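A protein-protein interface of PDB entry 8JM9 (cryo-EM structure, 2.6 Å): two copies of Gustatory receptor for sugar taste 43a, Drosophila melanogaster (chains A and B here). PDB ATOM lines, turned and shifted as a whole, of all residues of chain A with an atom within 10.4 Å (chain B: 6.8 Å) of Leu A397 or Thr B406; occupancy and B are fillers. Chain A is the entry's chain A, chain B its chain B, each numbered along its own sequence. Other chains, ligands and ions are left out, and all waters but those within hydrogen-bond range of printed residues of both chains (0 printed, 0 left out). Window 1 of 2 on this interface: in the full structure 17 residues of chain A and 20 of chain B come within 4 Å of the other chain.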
ATOM      1  N   SER A 289     -15.642  -2.415 -22.891  1.00  0.00           N
ATOM      2  CA  SER A 289     -16.610  -1.930 -21.916  1.00  0.00           C
ATOM      3  C   SER A 289     -16.746  -2.903 -20.754  1.00  0.00           C
ATOM      4  O   SER A 289     -16.586  -2.526 -19.593  1.00  0.00           O
ATOM      5  CB  SER A 289     -17.960  -1.707 -22.591  1.00  0.00           C
ATOM      6  OG  SER A 289     -18.771  -0.835 -21.828  1.00  0.00           O
ATOM      7  N   GLY A 293     -15.303  -0.944 -17.632  1.00  0.00           N
ATOM      8  CA  GLY A 293     -16.376   0.002 -17.393  1.00  0.00           C
ATOM      9  C   GLY A 293     -16.304   0.631 -16.019  1.00  0.00           C
ATOM     10  O   GLY A 293     -16.511   1.835 -15.871  1.00  0.00           O
ATOM     11  N   ILE A 294     -16.015  -0.170 -14.995  1.00  0.00           N
ATOM     12  CA  ILE A 294     -15.900   0.378 -13.650  1.00  0.00           C
ATOM     13  C   ILE A 294     -14.703   1.316 -13.562  1.00  0.00           C
ATOM     14  O   ILE A 294     -14.765   2.367 -12.912  1.00  0.00           O
ATOM     15  CB  ILE A 294     -15.821  -0.764 -12.619  1.00  0.00           C
ATOM     16  CG1 ILE A 294     -16.019  -0.223 -11.203  1.00  0.00           C
ATOM     17  CG2 ILE A 294     -14.504  -1.496 -12.731  1.00  0.00           C
ATOM     18  CD1 ILE A 294     -17.441   0.189 -10.901  1.00  0.00           C
ATOM     19  N   ALA A 295     -13.600   0.960 -14.222  1.00  0.00           N
ATOM     20  CA  ALA A 295     -12.434   1.834 -14.235  1.00  0.00           C
ATOM     21  C   ALA A 295     -12.758   3.164 -14.898  1.00  0.00           C
ATOM     22  O   ALA A 295     -12.389   4.227 -14.393  1.00  0.00           O
ATOM     23  CB  ALA A 295     -11.272   1.148 -14.951  1.00  0.00           C
ATOM     24  N   VAL A 296     -13.455   3.124 -16.035  1.00  0.00           N
ATOM     25  CA  VAL A 296     -13.821   4.357 -16.723  1.00  0.00           C
ATOM     26  C   VAL A 296     -14.788   5.170 -15.874  1.00  0.00           C
ATOM     27  O   VAL A 296     -14.707   6.401 -15.821  1.00  0.00           O
ATOM     28  CB  VAL A 296     -14.415   4.041 -18.106  1.00  0.00           C
ATOM     29  CG1 VAL A 296     -15.089   5.268 -18.689  1.00  0.00           C
ATOM     30  CG2 VAL A 296     -13.333   3.535 -19.037  1.00  0.00           C
ATOM     31  N   LEU A 297     -15.723   4.497 -15.204  1.00  0.00           N
ATOM     32  CA  LEU A 297     -16.680   5.196 -14.359  1.00  0.00           C
ATOM     33  C   LEU A 297     -15.974   5.936 -13.234  1.00  0.00           C
ATOM     34  O   LEU A 297     -16.270   7.103 -12.955  1.00  0.00           O
ATOM     35  CB  LEU A 297     -17.689   4.197 -13.795  1.00  0.00           C
ATOM     36  CG  LEU A 297     -18.789   4.765 -12.903  1.00  0.00           C
ATOM     37  CD1 LEU A 297     -19.692   5.690 -13.696  1.00  0.00           C
ATOM     38  CD2 LEU A 297     -19.586   3.639 -12.279  1.00  0.00           C
ATOM     39  N   PHE A 298     -15.023   5.273 -12.576  1.00  0.00           N
ATOM     40  CA  PHE A 298     -14.326   5.923 -11.475  1.00  0.00           C
ATOM     41  C   PHE A 298     -13.354   6.980 -11.978  1.00  0.00           C
ATOM     42  O   PHE A 298     -13.115   7.974 -11.288  1.00  0.00           O
ATOM     43  CB  PHE A 298     -13.612   4.882 -10.621  1.00  0.00           C
ATOM     44  CG  PHE A 298     -14.515   4.200  -9.638  1.00  0.00           C
ATOM     45  CD1 PHE A 298     -15.141   4.922  -8.638  1.00  0.00           C
ATOM     46  CD2 PHE A 298     -14.752   2.843  -9.721  1.00  0.00           C
ATOM     47  CE1 PHE A 298     -15.978   4.302  -7.739  1.00  0.00           C
ATOM     48  CE2 PHE A 298     -15.587   2.218  -8.823  1.00  0.00           C
ATOM     49  CZ  PHE A 298     -16.201   2.947  -7.832  1.00  0.00           C
ATOM     50  N   LEU A 300     -14.078   8.905 -14.532  1.00  0.00           N
ATOM     51  CA  LEU A 300     -14.976  10.033 -14.753  1.00  0.00           C
ATOM     52  C   LEU A 300     -15.359  10.694 -13.437  1.00  0.00           C
ATOM     53  O   LEU A 300     -15.435  11.925 -13.351  1.00  0.00           O
ATOM     54  CB  LEU A 300     -16.225   9.567 -15.497  1.00  0.00           C
ATOM     55  CG  LEU A 300     -16.015   9.137 -16.947  1.00  0.00           C
ATOM     56  CD1 LEU A 300     -17.260   8.451 -17.474  1.00  0.00           C
ATOM     57  CD2 LEU A 300     -15.649  10.324 -17.814  1.00  0.00           C
ATOM     58  N   VAL A 301     -15.618   9.894 -12.404  1.00  0.00           N
ATOM     59  CA  VAL A 301     -15.962  10.456 -11.102  1.00  0.00           C
ATOM     60  C   VAL A 301     -14.805  11.286 -10.562  1.00  0.00           C
ATOM     61  O   VAL A 301     -15.002  12.394 -10.043  1.00  0.00           O
ATOM     62  CB  VAL A 301     -16.356   9.334 -10.126  1.00  0.00           C
ATOM     63  CG1 VAL A 301     -16.311   9.832  -8.692  1.00  0.00           C
ATOM     64  CG2 VAL A 301     -17.733   8.802 -10.465  1.00  0.00           C
ATOM     65  N   LEU A 304     -14.580  14.566 -12.486  1.00  0.00           N
ATOM     66  CA  LEU A 304     -15.594  15.525 -12.063  1.00  0.00           C
ATOM     67  C   LEU A 304     -15.226  16.150 -10.725  1.00  0.00           C
ATOM     68  O   LEU A 304     -15.269  17.376 -10.564  1.00  0.00           O
ATOM     69  CB  LEU A 304     -16.958  14.841 -11.980  1.00  0.00           C
ATOM     70  CG  LEU A 304     -18.104  15.674 -11.403  1.00  0.00           C
ATOM     71  CD1 LEU A 304     -18.322  16.935 -12.215  1.00  0.00           C
ATOM     72  CD2 LEU A 304     -19.375  14.851 -11.351  1.00  0.00           C
ATOM     73  N   PHE A 392     -19.928   3.075 -26.056  1.00  0.00           N
ATOM     74  CA  PHE A 392     -19.242   2.541 -24.889  1.00  0.00           C
ATOM     75  C   PHE A 392     -20.065   2.831 -23.641  1.00  0.00           C
ATOM     76  O   PHE A 392     -20.501   3.966 -23.427  1.00  0.00           O
ATOM     77  CB  PHE A 392     -17.854   3.168 -24.773  1.00  0.00           C
ATOM     78  CG  PHE A 392     -17.040   2.655 -23.621  1.00  0.00           C
ATOM     79  CD1 PHE A 392     -17.225   3.154 -22.344  1.00  0.00           C
ATOM     80  CD2 PHE A 392     -16.074   1.690 -23.819  1.00  0.00           C
ATOM     81  CE1 PHE A 392     -16.472   2.685 -21.288  1.00  0.00           C
ATOM     82  CE2 PHE A 392     -15.319   1.224 -22.768  1.00  0.00           C
ATOM     83  CZ  PHE A 392     -15.518   1.723 -21.500  1.00  0.00           C
ATOM     84  N   SER A 393     -20.275   1.809 -22.819  1.00  0.00           N
ATOM     85  CA  SER A 393     -21.074   1.922 -21.608  1.00  0.00           C
ATOM     86  C   SER A 393     -20.180   1.745 -20.391  1.00  0.00           C
ATOM     87  O   SER A 393     -19.447   0.757 -20.293  1.00  0.00           O
ATOM     88  CB  SER A 393     -22.194   0.881 -21.599  1.00  0.00           C
ATOM     89  OG  SER A 393     -22.879   0.884 -20.361  1.00  0.00           O
ATOM     90  N   ALA A 394     -20.245   2.701 -19.465  1.00  0.00           N
ATOM     91  CA  ALA A 394     -19.462   2.646 -18.232  1.00  0.00           C
ATOM     92  C   ALA A 394     -20.269   1.886 -17.184  1.00  0.00           C
ATOM     93  O   ALA A 394     -20.928   2.460 -16.315  1.00  0.00           O
ATOM     94  CB  ALA A 394     -19.103   4.048 -17.761  1.00  0.00           C
ATOM     95  N   CYS A 395     -20.211   0.557 -17.277  1.00  0.00           N
ATOM     96  CA  CYS A 395     -20.895  -0.338 -16.348  1.00  0.00           C
ATOM     97  C   CYS A 395     -22.410  -0.174 -16.406  1.00  0.00           C
ATOM     98  O   CYS A 395     -23.120  -0.565 -15.478  1.00  0.00           O
ATOM     99  CB  CYS A 395     -20.400  -0.130 -14.912  1.00  0.00           C
ATOM    100  SG  CYS A 395     -18.912  -1.055 -14.503  1.00  0.00           S
ATOM    101  N   GLY A 396     -22.921   0.391 -17.494  1.00  0.00           N
ATOM    102  CA  GLY A 396     -24.336   0.660 -17.616  1.00  0.00           C
ATOM    103  C   GLY A 396     -24.804   1.903 -16.896  1.00  0.00           C
ATOM    104  O   GLY A 396     -25.970   2.285 -17.050  1.00  0.00           O
ATOM    105  N   LEU A 397     -23.934   2.544 -16.115  1.00  0.00           N
ATOM    106  CA  LEU A 397     -24.318   3.769 -15.424  1.00  0.00           C
ATOM    107  C   LEU A 397     -24.582   4.898 -16.410  1.00  0.00           C
ATOM    108  O   LEU A 397     -25.534   5.667 -16.242  1.00  0.00           O
ATOM    109  CB  LEU A 397     -23.227   4.171 -14.434  1.00  0.00           C
ATOM    110  CG  LEU A 397     -23.285   3.537 -13.044  1.00  0.00           C
ATOM    111  CD1 LEU A 397     -24.417   4.130 -12.238  1.00  0.00           C
ATOM    112  CD2 LEU A 397     -23.430   2.030 -13.134  1.00  0.00           C
ATOM    113  N   CYS A 398     -23.752   5.015 -17.440  1.00  0.00           N
ATOM    114  CA  CYS A 398     -23.889   6.094 -18.406  1.00  0.00           C
ATOM    115  C   CYS A 398     -23.246   5.668 -19.713  1.00  0.00           C
ATOM    116  O   CYS A 398     -22.466   4.715 -19.763  1.00  0.00           O
ATOM    117  CB  CYS A 398     -23.251   7.388 -17.894  1.00  0.00           C
ATOM    118  SG  CYS A 398     -21.465   7.293 -17.673  1.00  0.00           S
ATOM    119  N   ARG A 399     -23.590   6.391 -20.773  1.00  0.00           N
ATOM    120  CA  ARG A 399     -23.002   6.179 -22.085  1.00  0.00           C
ATOM    121  C   ARG A 399     -21.880   7.188 -22.284  1.00  0.00           C
ATOM    122  O   ARG A 399     -22.100   8.398 -22.173  1.00  0.00           O
ATOM    123  CB  ARG A 399     -24.067   6.323 -23.171  1.00  0.00           C
ATOM    124  CG  ARG A 399     -24.536   4.999 -23.746  1.00  0.00           C
ATOM    125  CD  ARG A 399     -25.176   5.178 -25.108  1.00  0.00           C
ATOM    126  NE  ARG A 399     -26.081   6.322 -25.150  1.00  0.00           N
ATOM    127  CZ  ARG A 399     -27.245   6.381 -24.518  1.00  0.00           C
ATOM    128  NH1 ARG A 399     -27.684   5.373 -23.779  1.00  0.00           N
ATOM    129  NH2 ARG A 399     -27.991   7.476 -24.632  1.00  0.00           N
ATOM    130  N   VAL A 400     -20.680   6.691 -22.564  1.00  0.00           N
ATOM    131  CA  VAL A 400     -19.485   7.526 -22.612  1.00  0.00           C
ATOM    132  C   VAL A 400     -19.368   8.123 -24.009  1.00  0.00           C
ATOM    133  O   VAL A 400     -19.026   7.429 -24.968  1.00  0.00           O
ATOM    134  CB  VAL A 400     -18.227   6.733 -22.240  1.00  0.00           C
ATOM    135  CG1 VAL A 400     -17.005   7.635 -22.269  1.00  0.00           C
ATOM    136  CG2 VAL A 400     -18.388   6.107 -20.869  1.00  0.00           C
ATOM    137  N   ASN A 401     -19.656   9.414 -24.117  1.00  0.00           N
ATOM    138  CA  ASN A 401     -19.477  10.167 -25.349  1.00  0.00           C
ATOM    139  C   ASN A 401     -19.358  11.637 -24.965  1.00  0.00           C
ATOM    140  O   ASN A 401     -19.201  11.973 -23.787  1.00  0.00           O
ATOM    141  CB  ASN A 401     -20.624   9.899 -26.329  1.00  0.00           C
ATOM    142  CG  ASN A 401     -21.979   9.991 -25.675  1.00  0.00           C
ATOM    143  OD1 ASN A 401     -22.135  10.626 -24.636  1.00  0.00           O
ATOM    144  ND2 ASN A 401     -22.971   9.353 -26.278  1.00  0.00           N
ATOM    145  N   THR A 403     -21.540  13.937 -24.827  1.00  0.00           N
ATOM    146  CA  THR A 403     -22.597  14.450 -23.965  1.00  0.00           C
ATOM    147  C   THR A 403     -22.203  14.400 -22.496  1.00  0.00           C
ATOM    148  O   THR A 403     -22.724  15.187 -21.695  1.00  0.00           O
ATOM    149  CB  THR A 403     -23.888  13.661 -24.179  1.00  0.00           C
ATOM    150  OG1 THR A 403     -24.316  13.800 -25.539  1.00  0.00           O
ATOM    151  CG2 THR A 403     -24.982  14.166 -23.254  1.00  0.00           C
ATOM    152  N   ILE A 404     -21.294  13.495 -22.126  1.00  0.00           N
ATOM    153  CA  ILE A 404     -20.784  13.488 -20.762  1.00  0.00           C
ATOM    154  C   ILE A 404     -20.090  14.803 -20.457  1.00  0.00           C
ATOM    155  O   ILE A 404     -20.101  15.267 -19.314  1.00  0.00           O
ATOM    156  CB  ILE A 404     -19.850  12.282 -20.542  1.00  0.00           C
ATOM    157  CG1 ILE A 404     -20.675  11.062 -20.131  1.00  0.00           C
ATOM    158  CG2 ILE A 404     -18.782  12.605 -19.496  1.00  0.00           C
ATOM    159  CD1 ILE A 404     -19.858   9.843 -19.792  1.00  0.00           C
ATOM    160  N   SER A 407     -22.867  17.126 -19.478  1.00  0.00           N
ATOM    161  CA  SER A 407     -23.332  16.812 -18.131  1.00  0.00           C
ATOM    162  C   SER A 407     -22.342  17.299 -17.081  1.00  0.00           C
ATOM    163  O   SER A 407     -22.736  17.865 -16.053  1.00  0.00           O
ATOM    164  CB  SER A 407     -23.557  15.308 -17.993  1.00  0.00           C
ATOM    165  OG  SER A 407     -24.728  14.905 -18.681  1.00  0.00           O
ATOM    166  N   PHE A 408     -21.048  17.085 -17.322  1.00  0.00           N
ATOM    167  CA  PHE A 408     -20.029  17.557 -16.394  1.00  0.00           C
ATOM    168  C   PHE A 408     -20.037  19.072 -16.300  1.00  0.00           C
ATOM    169  O   PHE A 408     -19.874  19.631 -15.214  1.00  0.00           O
ATOM    170  CB  PHE A 408     -18.651  17.062 -16.833  1.00  0.00           C
ATOM    171  CG  PHE A 408     -18.308  15.693 -16.330  1.00  0.00           C
ATOM    172  CD1 PHE A 408     -19.291  14.739 -16.148  1.00  0.00           C
ATOM    173  CD2 PHE A 408     -17.000  15.360 -16.040  1.00  0.00           C
ATOM    174  CE1 PHE A 408     -18.975  13.482 -15.686  1.00  0.00           C
ATOM    175  CE2 PHE A 408     -16.680  14.106 -15.579  1.00  0.00           C
ATOM    176  CZ  PHE A 408     -17.669  13.166 -15.402  1.00  0.00           C
ATOM    177  N   ALA A 411     -23.040  20.071 -14.136  1.00  0.00           N
ATOM    178  CA  ALA A 411     -22.810  19.772 -12.727  1.00  0.00           C
ATOM    179  C   ALA A 411     -21.783  20.718 -12.122  1.00  0.00           C
ATOM    180  O   ALA A 411     -21.960  21.206 -10.999  1.00  0.00           O
ATOM    181  CB  ALA A 411     -22.358  18.322 -12.570  1.00  0.00           C
ATOM    182  N   TYR A 415     -22.470  23.273  -8.990  1.00  0.00           N
ATOM    183  CA  TYR A 415     -21.707  23.181  -7.751  1.00  0.00           C
ATOM    184  C   TYR A 415     -20.907  24.450  -7.504  1.00  0.00           C
ATOM    185  O   TYR A 415     -20.838  24.939  -6.371  1.00  0.00           O
ATOM    186  CB  TYR A 415     -20.778  21.971  -7.790  1.00  0.00           C
ATOM    187  CG  TYR A 415     -21.480  20.653  -8.017  1.00  0.00           C
ATOM    188  CD1 TYR A 415     -22.773  20.444  -7.568  1.00  0.00           C
ATOM    189  CD2 TYR A 415     -20.845  19.618  -8.684  1.00  0.00           C
ATOM    190  CE1 TYR A 415     -23.414  19.243  -7.776  1.00  0.00           C
ATOM    191  CE2 TYR A 415     -21.476  18.414  -8.896  1.00  0.00           C
ATOM    192  CZ  TYR A 415     -22.761  18.231  -8.442  1.00  0.00           C
ATOM    193  OH  TYR A 415     -23.392  17.030  -8.655  1.00  0.00           O
ATOM    194  N   GLU B 346     -30.707  -3.505  -9.938  1.00  0.00           N
ATOM    195  CA  GLU B 346     -29.943  -4.499 -10.688  1.00  0.00           C
ATOM    196  C   GLU B 346     -30.822  -5.528 -11.379  1.00  0.00           C
ATOM    197  O   GLU B 346     -30.545  -5.859 -12.544  1.00  0.00           O
ATOM    198  CB  GLU B 346     -28.949  -5.186  -9.746  1.00  0.00           C
ATOM    199  CG  GLU B 346     -27.501  -4.736  -9.884  1.00  0.00           C
ATOM    200  CD  GLU B 346     -27.011  -4.736 -11.317  1.00  0.00           C
ATOM    201  OE1 GLU B 346     -26.223  -3.837 -11.673  1.00  0.00           O
ATOM    202  OE2 GLU B 346     -27.412  -5.634 -12.085  1.00  0.00           O
ATOM    203  N   HIS B 349     -32.220  -4.039 -14.622  1.00  0.00           N
ATOM    204  CA  HIS B 349     -31.159  -3.823 -15.596  1.00  0.00           C
ATOM    205  C   HIS B 349     -30.728  -5.136 -16.231  1.00  0.00           C
ATOM    206  O   HIS B 349     -30.555  -5.218 -17.452  1.00  0.00           O
ATOM    207  CB  HIS B 349     -29.970  -3.139 -14.924  1.00  0.00           C
ATOM    208  CG  HIS B 349     -28.821  -2.884 -15.846  1.00  0.00           C
ATOM    209  ND1 HIS B 349     -28.684  -1.711 -16.556  1.00  0.00           N
ATOM    210  CD2 HIS B 349     -27.753  -3.649 -16.172  1.00  0.00           C
ATOM    211  CE1 HIS B 349     -27.581  -1.765 -17.281  1.00  0.00           C
ATOM    212  NE2 HIS B 349     -26.998  -2.930 -17.067  1.00  0.00           N
ATOM    213  N   ASN B 401     -33.283   1.003 -14.341  1.00  0.00           N
ATOM    214  CA  ASN B 401     -32.044   0.353 -14.738  1.00  0.00           C
ATOM    215  C   ASN B 401     -30.910   1.058 -14.002  1.00  0.00           C
ATOM    216  O   ASN B 401     -31.147   1.845 -13.080  1.00  0.00           O
ATOM    217  CB  ASN B 401     -31.872   0.378 -16.260  1.00  0.00           C
ATOM    218  CG  ASN B 401     -32.136   1.740 -16.851  1.00  0.00           C
ATOM    219  OD1 ASN B 401     -32.054   2.752 -16.162  1.00  0.00           O
ATOM    220  ND2 ASN B 401     -32.461   1.774 -18.135  1.00  0.00           N
ATOM    221  N   ARG B 402     -29.673   0.780 -14.402  1.00  0.00           N
ATOM    222  CA  ARG B 402     -28.526   1.336 -13.700  1.00  0.00           C
ATOM    223  C   ARG B 402     -28.386   2.842 -13.875  1.00  0.00           C
ATOM    224  O   ARG B 402     -27.702   3.475 -13.066  1.00  0.00           O
ATOM    225  CB  ARG B 402     -27.246   0.646 -14.163  1.00  0.00           C
ATOM    226  CG  ARG B 402     -26.945  -0.626 -13.407  1.00  0.00           C
ATOM    227  CD  ARG B 402     -25.586  -1.167 -13.776  1.00  0.00           C
ATOM    228  NE  ARG B 402     -25.453  -2.575 -13.428  1.00  0.00           N
ATOM    229  CZ  ARG B 402     -24.537  -3.386 -13.937  1.00  0.00           C
ATOM    230  NH1 ARG B 402     -23.655  -2.961 -14.825  1.00  0.00           N
ATOM    231  NH2 ARG B 402     -24.507  -4.655 -13.547  1.00  0.00           N
ATOM    232  N   THR B 403     -29.005   3.433 -14.898  1.00  0.00           N
ATOM    233  CA  THR B 403     -28.982   4.885 -15.022  1.00  0.00           C
ATOM    234  C   THR B 403     -29.686   5.564 -13.856  1.00  0.00           C
ATOM    235  O   THR B 403     -29.372   6.718 -13.540  1.00  0.00           O
ATOM    236  CB  THR B 403     -29.628   5.317 -16.337  1.00  0.00           C
ATOM    237  OG1 THR B 403     -28.897   4.764 -17.437  1.00  0.00           O
ATOM    238  CG2 THR B 403     -29.641   6.832 -16.453  1.00  0.00           C
ATOM    239  N   ILE B 404     -30.628   4.873 -13.210  1.00  0.00           N
ATOM    240  CA  ILE B 404     -31.242   5.422 -12.010  1.00  0.00           C
ATOM    241  C   ILE B 404     -30.190   5.636 -10.937  1.00  0.00           C
ATOM    242  O   ILE B 404     -30.302   6.558 -10.125  1.00  0.00           O
ATOM    243  CB  ILE B 404     -32.382   4.506 -11.521  1.00  0.00           C
ATOM    244  CG1 ILE B 404     -33.683   4.881 -12.233  1.00  0.00           C
ATOM    245  CG2 ILE B 404     -32.538   4.597 -10.002  1.00  0.00           C
ATOM    246  CD1 ILE B 404     -34.892   4.117 -11.763  1.00  0.00           C
ATOM    247  N   LEU B 405     -29.155   4.797 -10.908  1.00  0.00           N
ATOM    248  CA  LEU B 405     -28.065   5.022  -9.965  1.00  0.00           C
ATOM    249  C   LEU B 405     -27.345   6.330 -10.262  1.00  0.00           C
ATOM    250  O   LEU B 405     -27.002   7.075  -9.340  1.00  0.00           O
ATOM    251  CB  LEU B 405     -27.084   3.852 -10.002  1.00  0.00           C
ATOM    252  CG  LEU B 405     -27.664   2.484  -9.651  1.00  0.00           C
ATOM    253  CD1 LEU B 405     -26.613   1.407  -9.838  1.00  0.00           C
ATOM    254  CD2 LEU B 405     -28.197   2.471  -8.232  1.00  0.00           C
ATOM    255  N   THR B 406     -27.105   6.627 -11.540  1.00  0.00           N
ATOM    256  CA  THR B 406     -26.480   7.898 -11.893  1.00  0.00           C
ATOM    257  C   THR B 406     -27.368   9.074 -11.507  1.00  0.00           C
ATOM    258  O   THR B 406     -26.882  10.085 -10.984  1.00  0.00           O
ATOM    259  CB  THR B 406     -26.175   7.935 -13.390  1.00  0.00           C
ATOM    260  OG1 THR B 406     -25.536   6.715 -13.781  1.00  0.00           O
ATOM    261  CG2 THR B 406     -25.267   9.104 -13.721  1.00  0.00           C
ATOM    262  N   SER B 407     -28.672   8.965 -11.762  1.00  0.00           N
ATOM    263  CA  SER B 407     -29.584  10.040 -11.386  1.00  0.00           C
ATOM    264  C   SER B 407     -29.599  10.244  -9.876  1.00  0.00           C
ATOM    265  O   SER B 407     -29.581  11.382  -9.391  1.00  0.00           O
ATOM    266  CB  SER B 407     -30.991   9.734 -11.896  1.00  0.00           C
ATOM    267  OG  SER B 407     -31.073   9.917 -13.297  1.00  0.00           O
ATOM    268  N   PHE B 408     -29.634   9.148  -9.116  1.00  0.00           N
ATOM    269  CA  PHE B 408     -29.606   9.248  -7.664  1.00  0.00           C
ATOM    270  C   PHE B 408     -28.303   9.864  -7.185  1.00  0.00           C
ATOM    271  O   PHE B 408     -28.299  10.667  -6.251  1.00  0.00           O
ATOM    272  CB  PHE B 408     -29.796   7.865  -7.041  1.00  0.00           C
ATOM    273  CG  PHE B 408     -31.230   7.469  -6.868  1.00  0.00           C
ATOM    274  CD1 PHE B 408     -32.195   7.896  -7.760  1.00  0.00           C
ATOM    275  CD2 PHE B 408     -31.614   6.668  -5.811  1.00  0.00           C
ATOM    276  CE1 PHE B 408     -33.512   7.531  -7.601  1.00  0.00           C
ATOM    277  CE2 PHE B 408     -32.929   6.302  -5.648  1.00  0.00           C
ATOM    278  CZ  PHE B 408     -33.879   6.733  -6.545  1.00  0.00           C
ATOM    279  N   ALA B 409     -27.183   9.488  -7.801  1.00  0.00           N
ATOM    280  CA  ALA B 409     -25.905  10.068  -7.415  1.00  0.00           C
ATOM    281  C   ALA B 409     -25.892  11.568  -7.664  1.00  0.00           C
ATOM    282  O   ALA B 409     -25.436  12.341  -6.817  1.00  0.00           O
ATOM    283  CB  ALA B 409     -24.768   9.391  -8.177  1.00  0.00           C
ATOM    284  N   SER B 410     -26.402  12.001  -8.818  1.00  0.00           N
ATOM    285  CA  SER B 410     -26.441  13.429  -9.113  1.00  0.00           C
ATOM    286  C   SER B 410     -27.319  14.171  -8.112  1.00  0.00           C
ATOM    287  O   SER B 410     -26.930  15.219  -7.579  1.00  0.00           O
ATOM    288  CB  SER B 410     -26.946  13.649 -10.538  1.00  0.00           C
ATOM    289  OG  SER B 410     -26.751  14.991 -10.944  1.00  0.00           O
ATOM    290  N   ALA B 411     -28.511  13.636  -7.839  1.00  0.00           N
ATOM    291  CA  ALA B 411     -29.415  14.294  -6.903  1.00  0.00           C
ATOM    292  C   ALA B 411     -28.817  14.350  -5.504  1.00  0.00           C
ATOM    293  O   ALA B 411     -28.904  15.378  -4.822  1.00  0.00           O
ATOM    294  CB  ALA B 411     -30.759  13.571  -6.880  1.00  0.00           C
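Of the 26 printed residues of chain A, 3 touch a printed residue of chain B. Hydrophobic or aromatic side chains of chain A within 4 Å of the printed part of chain B: Leu A397. Among the printed residues, 7 pairs touch across the chains. Among the printed residues, no Asp or Glu carboxylate lies within 4 Å of a Lys or Arg side-chain nitrogen of the other chain.
Among the printed residues, merely in contact across the chains: Gly A396 with Arg B402, Gly A396 with Thr B403, Leu A397 with Arg B402, Leu A397 with Thr B403 and Leu A397 with Leu B405.
Leu A397 touches just these residues of chain B: Arg B402 (3.5 Å), Thr B403 (3.7 Å), Leu B405 (3.5 Å) and Thr B406 (2.7 Å). Thr B406 touches just one residue of chain A: Leu A397 (2.7 Å). Thr B403 touches two residues of chain A. Of chain A, only Leu A397 comes within 4 Å of Leu B405. Ala B409 touches none of the printed residues of chain A. No residue of chain A comes within 4 Å of Ser B410. Of the printed residues of chain B, Gly A396 touches Arg B402 and Thr B403. Of the printed residues of chain A, Arg B402 touches Cys A395, Gly A396 and Leu A397. Gly A293 touches none of the printed residues of chain B. The nearest residue of chain B that does not touch Leu A397 is His B349 (5.8 Å).
Positions printed for both chains: 401, 403, 404, 407, 408 and 411. Of the 7 pairs that touch across the chains among the printed residues, none has its exchanged pair printed and touching as well.
NH1 of Arg B402 lies within hydrogen-bond range of O of Cys A395 (2.5 Å). O of Leu A397 is in hydrogen-bond range of OG1 of Thr B406 (2.7 Å).
The side-chain sulfur (SG) of Cys A395 lies within hydrogen-bond range of the backbone NH (N) of Ile A294, at 3.1 Å. The side-chain hydroxyl (OG) of Ser A393 lies within hydrogen-bond range of the backbone NH (N) of Gly A396, 2.9 Å away. NH2 of Arg B402 lies within salt-bridge range of OE1 of Glu B346 (2.7 Å). A ring nitrogen (ND1) of His B349 lies within hydrogen-bond range of the backbone NH of Arg B402 (3.4 Å). The side-chain amide oxygen (OD1) of Asn B401 lies close to the backbone NH (N) of Thr B403, 3.4 Å away.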
